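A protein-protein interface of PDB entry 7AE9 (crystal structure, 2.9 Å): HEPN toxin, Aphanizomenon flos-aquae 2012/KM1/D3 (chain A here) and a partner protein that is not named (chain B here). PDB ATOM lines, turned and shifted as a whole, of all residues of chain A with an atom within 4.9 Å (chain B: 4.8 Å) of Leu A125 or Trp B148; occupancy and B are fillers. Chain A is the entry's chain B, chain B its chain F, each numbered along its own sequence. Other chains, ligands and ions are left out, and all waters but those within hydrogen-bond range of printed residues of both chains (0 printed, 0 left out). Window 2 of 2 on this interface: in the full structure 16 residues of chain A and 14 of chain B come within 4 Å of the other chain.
The side-chain carboxylate of Asp A21 is in salt-bridge range of the guanidinium group of Arg B147, 2.6 Å away. NE1 of Trp B148 lies within hydrogen-bond range of OD1 of Asp A21.
N of Val B150 sits at hydrogen-bond distance from O of Leu B145, at 3.3 Å.
Phe B144 touches Leu A20 (CZ to CD1, 3.7 Å). Trp B148 touches Leu A20. Lys A24 touches Trp B148. Leu A125 touches Trp B148. CG of Pro A129 touches CE3 of Trp B148, at 3.6 Å. Pro A129 touches Val B150 (CB to CG1, 3.9 Å).
Ala A124 touches none of the printed residues of chain B. Of chain B, only Trp B148 comes within 4 Å of Leu A125. Gln B146 touches none of the printed residues of chain A. Printed residues of chain A within 4 Å of Arg B147: Asp A21. Of the printed residues of chain A, Val B150 touches Pro A129 (3.9 Å). The nearest printed residue of chain B that does not touch Leu A125 is Val B150 (6.6 Å). The nearest printed residue of chain A that does not touch Trp B148 is Leu A23 (5.9 Å).
Of the 13 printed residues of chain A, 5 touch a printed residue of chain B. Printed residues of chain A that touch a printed residue of chain B: Leu A20, Asp A21, Lys A24, Leu A125 and Pro A129. Of the 7 printed residues of chain B, 4 touch a printed residue of chain A. Printed residues of chain B that touch a printed residue of chain A: Phe B144, Arg B147, Trp B148 and Val B150. Among the printed residues, 8 pairs touch across the chains. Among the printed residues, Asp or Glu carboxylates within 4 Å of a Lys or Arg side-chain nitrogen of the other chain: Asp A21 with Arg B147.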
ATOM      1  N   LEU A  20      -3.474   1.661  24.595  1.00  0.00           N
ATOM      2  CA  LEU A  20      -4.415   0.560  24.792  1.00  0.00           C
ATOM      3  C   LEU A  20      -3.944  -0.718  24.109  1.00  0.00           C
ATOM      4  O   LEU A  20      -4.119  -1.815  24.651  1.00  0.00           O
ATOM      5  CB  LEU A  20      -5.793   0.959  24.288  1.00  0.00           C
ATOM      6  CG  LEU A  20      -6.617   1.848  25.210  1.00  0.00           C
ATOM      7  CD1 LEU A  20      -7.822   2.425  24.481  1.00  0.00           C
ATOM      8  CD2 LEU A  20      -7.071   1.020  26.379  1.00  0.00           C
ATOM      9  N   ASP A  21      -3.348  -0.604  22.917  1.00  0.00           N
ATOM     10  CA  ASP A  21      -2.841  -1.800  22.251  1.00  0.00           C
ATOM     11  C   ASP A  21      -1.770  -2.468  23.089  1.00  0.00           C
ATOM     12  O   ASP A  21      -1.675  -3.700  23.126  1.00  0.00           O
ATOM     13  CB  ASP A  21      -2.312  -1.469  20.852  1.00  0.00           C
ATOM     14  CG  ASP A  21      -3.411  -1.494  19.777  1.00  0.00           C
ATOM     15  OD1 ASP A  21      -4.367  -2.300  19.908  1.00  0.00           O
ATOM     16  OD2 ASP A  21      -3.316  -0.716  18.802  1.00  0.00           O
ATOM     17  N   LEU A  23      -1.603  -2.012  26.516  1.00  0.00           N
ATOM     18  CA  LEU A  23      -2.297  -2.477  27.712  1.00  0.00           C
ATOM     19  C   LEU A  23      -3.039  -3.782  27.466  1.00  0.00           C
ATOM     20  O   LEU A  23      -3.209  -4.577  28.394  1.00  0.00           O
ATOM     21  CB  LEU A  23      -3.268  -1.403  28.211  1.00  0.00           C
ATOM     22  CG  LEU A  23      -3.994  -1.712  29.527  1.00  0.00           C
ATOM     23  CD1 LEU A  23      -3.012  -2.033  30.634  1.00  0.00           C
ATOM     24  CD2 LEU A  23      -4.844  -0.537  29.937  1.00  0.00           C
ATOM     25  N   LYS A  24      -3.457  -4.048  26.225  1.00  0.00           N
ATOM     26  CA  LYS A  24      -4.192  -5.279  25.964  1.00  0.00           C
ATOM     27  C   LYS A  24      -3.331  -6.513  26.182  1.00  0.00           C
ATOM     28  O   LYS A  24      -3.870  -7.612  26.339  1.00  0.00           O
ATOM     29  CB  LYS A  24      -4.747  -5.293  24.541  1.00  0.00           C
ATOM     30  CG  LYS A  24      -5.837  -6.333  24.306  1.00  0.00           C
ATOM     31  CD  LYS A  24      -5.971  -6.689  22.829  1.00  0.00           C
ATOM     32  CE  LYS A  24      -7.376  -6.412  22.309  1.00  0.00           C
ATOM     33  NZ  LYS A  24      -7.411  -6.214  20.819  1.00  0.00           N
ATOM     34  N   GLU A  27      -4.557  -8.469  29.227  1.00  0.00           N
ATOM     35  CA  GLU A  27      -5.984  -8.764  29.328  1.00  0.00           C
ATOM     36  C   GLU A  27      -6.241 -10.109  29.998  1.00  0.00           C
ATOM     37  O   GLU A  27      -7.226 -10.264  30.728  1.00  0.00           O
ATOM     38  CB  GLU A  27      -6.631  -8.726  27.941  1.00  0.00           C
ATOM     39  N   ILE A 121      -7.086  -2.118  35.144  1.00  0.00           N
ATOM     40  CA  ILE A 121      -6.716  -2.613  33.819  1.00  0.00           C
ATOM     41  C   ILE A 121      -7.959  -3.013  33.045  1.00  0.00           C
ATOM     42  O   ILE A 121      -8.194  -2.542  31.929  1.00  0.00           O
ATOM     43  CB  ILE A 121      -5.734  -3.789  33.934  1.00  0.00           C
ATOM     44  CG1 ILE A 121      -4.400  -3.341  34.540  1.00  0.00           C
ATOM     45  CG2 ILE A 121      -5.567  -4.484  32.592  1.00  0.00           C
ATOM     46  CD1 ILE A 121      -3.448  -4.505  34.813  1.00  0.00           C
ATOM     47  N   SER A 122      -8.785  -3.876  33.641  1.00  0.00           N
ATOM     48  CA  SER A 122     -10.014  -4.308  32.986  1.00  0.00           C
ATOM     49  C   SER A 122     -10.955  -3.140  32.750  1.00  0.00           C
ATOM     50  O   SER A 122     -11.649  -3.083  31.724  1.00  0.00           O
ATOM     51  CB  SER A 122     -10.714  -5.356  33.839  1.00  0.00           C
ATOM     52  OG  SER A 122     -10.275  -6.642  33.488  1.00  0.00           O
ATOM     53  N   PHE A 123     -10.984  -2.193  33.683  1.00  0.00           N
ATOM     54  CA  PHE A 123     -11.830  -1.026  33.505  1.00  0.00           C
ATOM     55  C   PHE A 123     -11.430  -0.279  32.245  1.00  0.00           C
ATOM     56  O   PHE A 123     -12.263  -0.008  31.374  1.00  0.00           O
ATOM     57  CB  PHE A 123     -11.730  -0.122  34.729  1.00  0.00           C
ATOM     58  CG  PHE A 123     -12.451   1.177  34.581  1.00  0.00           C
ATOM     59  CD1 PHE A 123     -13.806   1.248  34.846  1.00  0.00           C
ATOM     60  CD2 PHE A 123     -11.789   2.316  34.158  1.00  0.00           C
ATOM     61  CE1 PHE A 123     -14.491   2.432  34.718  1.00  0.00           C
ATOM     62  CE2 PHE A 123     -12.468   3.502  34.022  1.00  0.00           C
ATOM     63  CZ  PHE A 123     -13.824   3.564  34.302  1.00  0.00           C
ATOM     64  N   ALA A 124     -10.137   0.012  32.109  1.00  0.00           N
ATOM     65  CA  ALA A 124      -9.671   0.798  30.975  1.00  0.00           C
ATOM     66  C   ALA A 124      -9.888   0.061  29.660  1.00  0.00           C
ATOM     67  O   ALA A 124     -10.253   0.680  28.652  1.00  0.00           O
ATOM     68  CB  ALA A 124      -8.191   1.143  31.153  1.00  0.00           C
ATOM     69  N   LEU A 125      -9.689  -1.258  29.654  1.00  0.00           N
ATOM     70  CA  LEU A 125      -9.848  -2.026  28.428  1.00  0.00           C
ATOM     71  C   LEU A 125     -11.298  -2.097  27.958  1.00  0.00           C
ATOM     72  O   LEU A 125     -11.550  -2.458  26.805  1.00  0.00           O
ATOM     73  CB  LEU A 125      -9.284  -3.427  28.635  1.00  0.00           C
ATOM     74  CG  LEU A 125      -7.765  -3.426  28.787  1.00  0.00           C
ATOM     75  CD1 LEU A 125      -7.242  -4.825  29.106  1.00  0.00           C
ATOM     76  CD2 LEU A 125      -7.115  -2.879  27.519  1.00  0.00           C
ATOM     77  N   GLN A 126     -12.258  -1.766  28.812  1.00  0.00           N
ATOM     78  CA  GLN A 126     -13.651  -1.776  28.402  1.00  0.00           C
ATOM     79  C   GLN A 126     -14.185  -0.385  28.124  1.00  0.00           C
ATOM     80  O   GLN A 126     -14.989  -0.219  27.202  1.00  0.00           O
ATOM     81  CB  GLN A 126     -14.530  -2.448  29.465  1.00  0.00           C
ATOM     82  N   GLN A 127     -13.737   0.620  28.872  1.00  0.00           N
ATOM     83  CA  GLN A 127     -14.329   1.944  28.754  1.00  0.00           C
ATOM     84  C   GLN A 127     -13.616   2.845  27.749  1.00  0.00           C
ATOM     85  O   GLN A 127     -14.275   3.642  27.071  1.00  0.00           O
ATOM     86  CB  GLN A 127     -14.348   2.626  30.127  1.00  0.00           C
ATOM     87  CG  GLN A 127     -15.020   1.804  31.199  1.00  0.00           C
ATOM     88  CD  GLN A 127     -16.450   1.449  30.844  1.00  0.00           C
ATOM     89  OE1 GLN A 127     -16.776   0.281  30.621  1.00  0.00           O
ATOM     90  NE2 GLN A 127     -17.314   2.454  30.793  1.00  0.00           N
ATOM     91  N   PRO A 129     -11.827   2.235  24.778  1.00  0.00           N
ATOM     92  CA  PRO A 129     -12.245   2.083  23.372  1.00  0.00           C
ATOM     93  C   PRO A 129     -13.558   2.790  23.067  1.00  0.00           C
ATOM     94  O   PRO A 129     -13.695   3.405  22.001  1.00  0.00           O
ATOM     95  CB  PRO A 129     -12.348   0.566  23.202  1.00  0.00           C
ATOM     96  CG  PRO A 129     -11.317   0.044  24.121  1.00  0.00           C
ATOM     97  CD  PRO A 129     -11.354   0.951  25.329  1.00  0.00           C
ATOM     98  N   PHE B 144      -7.757   1.223  14.643  1.00  0.00           N
ATOM     99  CA  PHE B 144      -7.858   0.804  16.030  1.00  0.00           C
ATOM    100  C   PHE B 144      -9.274   0.371  16.338  1.00  0.00           C
ATOM    101  O   PHE B 144      -9.501  -0.716  16.877  1.00  0.00           O
ATOM    102  CB  PHE B 144      -7.441   1.940  16.966  1.00  0.00           C
ATOM    103  CG  PHE B 144      -7.833   1.708  18.408  1.00  0.00           C
ATOM    104  CD1 PHE B 144      -7.007   0.987  19.256  1.00  0.00           C
ATOM    105  CD2 PHE B 144      -9.040   2.191  18.904  1.00  0.00           C
ATOM    106  CE1 PHE B 144      -7.373   0.744  20.573  1.00  0.00           C
ATOM    107  CE2 PHE B 144      -9.409   1.962  20.209  1.00  0.00           C
ATOM    108  CZ  PHE B 144      -8.574   1.231  21.053  1.00  0.00           C
ATOM    109  N   LEU B 145     -10.243   1.215  15.981  1.00  0.00           N
ATOM    110  CA  LEU B 145     -11.635   0.912  16.262  1.00  0.00           C
ATOM    111  C   LEU B 145     -12.063  -0.360  15.555  1.00  0.00           C
ATOM    112  O   LEU B 145     -12.858  -1.141  16.086  1.00  0.00           O
ATOM    113  CB  LEU B 145     -12.504   2.087  15.844  1.00  0.00           C
ATOM    114  CG  LEU B 145     -12.339   3.379  16.637  1.00  0.00           C
ATOM    115  CD1 LEU B 145     -13.093   4.526  15.972  1.00  0.00           C
ATOM    116  CD2 LEU B 145     -12.843   3.192  18.045  1.00  0.00           C
ATOM    117  N   GLN B 146     -11.546  -0.587  14.355  1.00  0.00           N
ATOM    118  CA  GLN B 146     -11.865  -1.818  13.649  1.00  0.00           C
ATOM    119  C   GLN B 146     -11.201  -3.023  14.301  1.00  0.00           C
ATOM    120  O   GLN B 146     -11.846  -4.060  14.504  1.00  0.00           O
ATOM    121  CB  GLN B 146     -11.448  -1.697  12.189  1.00  0.00           C
ATOM    122  CG  GLN B 146     -11.068  -3.012  11.571  1.00  0.00           C
ATOM    123  CD  GLN B 146     -10.500  -2.837  10.188  1.00  0.00           C
ATOM    124  OE1 GLN B 146     -10.965  -2.000   9.409  1.00  0.00           O
ATOM    125  NE2 GLN B 146      -9.468  -3.619   9.875  1.00  0.00           N
ATOM    126  N   ARG B 147      -9.935  -2.887  14.702  1.00  0.00           N
ATOM    127  CA  ARG B 147      -9.221  -4.042  15.229  1.00  0.00           C
ATOM    128  C   ARG B 147      -9.810  -4.479  16.559  1.00  0.00           C
ATOM    129  O   ARG B 147      -9.743  -5.662  16.906  1.00  0.00           O
ATOM    130  CB  ARG B 147      -7.733  -3.718  15.381  1.00  0.00           C
ATOM    131  CG  ARG B 147      -6.938  -3.743  14.074  1.00  0.00           C
ATOM    132  CD  ARG B 147      -5.436  -3.557  14.290  1.00  0.00           C
ATOM    133  NE  ARG B 147      -5.144  -2.244  14.854  1.00  0.00           N
ATOM    134  CZ  ARG B 147      -4.788  -2.047  16.121  1.00  0.00           C
ATOM    135  NH1 ARG B 147      -4.666  -3.076  16.941  1.00  0.00           N
ATOM    136  NH2 ARG B 147      -4.562  -0.824  16.571  1.00  0.00           N
ATOM    137  N   TRP B 148     -10.410  -3.542  17.293  1.00  0.00           N
ATOM    138  CA  TRP B 148     -10.994  -3.778  18.605  1.00  0.00           C
ATOM    139  C   TRP B 148     -12.496  -4.050  18.585  1.00  0.00           C
ATOM    140  O   TRP B 148     -13.068  -4.351  19.641  1.00  0.00           O
ATOM    141  CB  TRP B 148     -10.710  -2.574  19.510  1.00  0.00           C
ATOM    142  CG  TRP B 148      -9.319  -2.539  20.047  1.00  0.00           C
ATOM    143  CD1 TRP B 148      -8.171  -2.452  19.340  1.00  0.00           C
ATOM    144  CD2 TRP B 148      -8.942  -2.610  21.421  1.00  0.00           C
ATOM    145  NE1 TRP B 148      -7.094  -2.461  20.183  1.00  0.00           N
ATOM    146  CE2 TRP B 148      -7.544  -2.560  21.471  1.00  0.00           C
ATOM    147  CE3 TRP B 148      -9.655  -2.716  22.616  1.00  0.00           C
ATOM    148  CZ2 TRP B 148      -6.842  -2.606  22.665  1.00  0.00           C
ATOM    149  CZ3 TRP B 148      -8.958  -2.754  23.791  1.00  0.00           C
ATOM    150  CH2 TRP B 148      -7.566  -2.699  23.809  1.00  0.00           C
ATOM    151  N   GLY B 149     -13.146  -3.955  17.431  1.00  0.00           N
ATOM    152  CA  GLY B 149     -14.553  -4.295  17.369  1.00  0.00           C
ATOM    153  C   GLY B 149     -15.442  -3.400  18.200  1.00  0.00           C
ATOM    154  O   GLY B 149     -16.421  -3.877  18.784  1.00  0.00           O
ATOM    155  N   VAL B 150     -15.165  -2.104  18.215  1.00  0.00           N
ATOM    156  CA  VAL B 150     -16.004  -1.159  18.948  1.00  0.00           C
ATOM    157  C   VAL B 150     -16.586  -0.061  18.047  1.00  0.00           C
ATOM    158  O   VAL B 150     -16.323   0.001  16.836  1.00  0.00           O
ATOM    159  CB  VAL B 150     -15.209  -0.521  20.097  1.00  0.00           C
ATOM    160  CG1 VAL B 150     -14.858  -1.568  21.146  1.00  0.00           C
ATOM    161  CG2 VAL B 150     -13.946   0.139  19.566  1.00  0.00           C
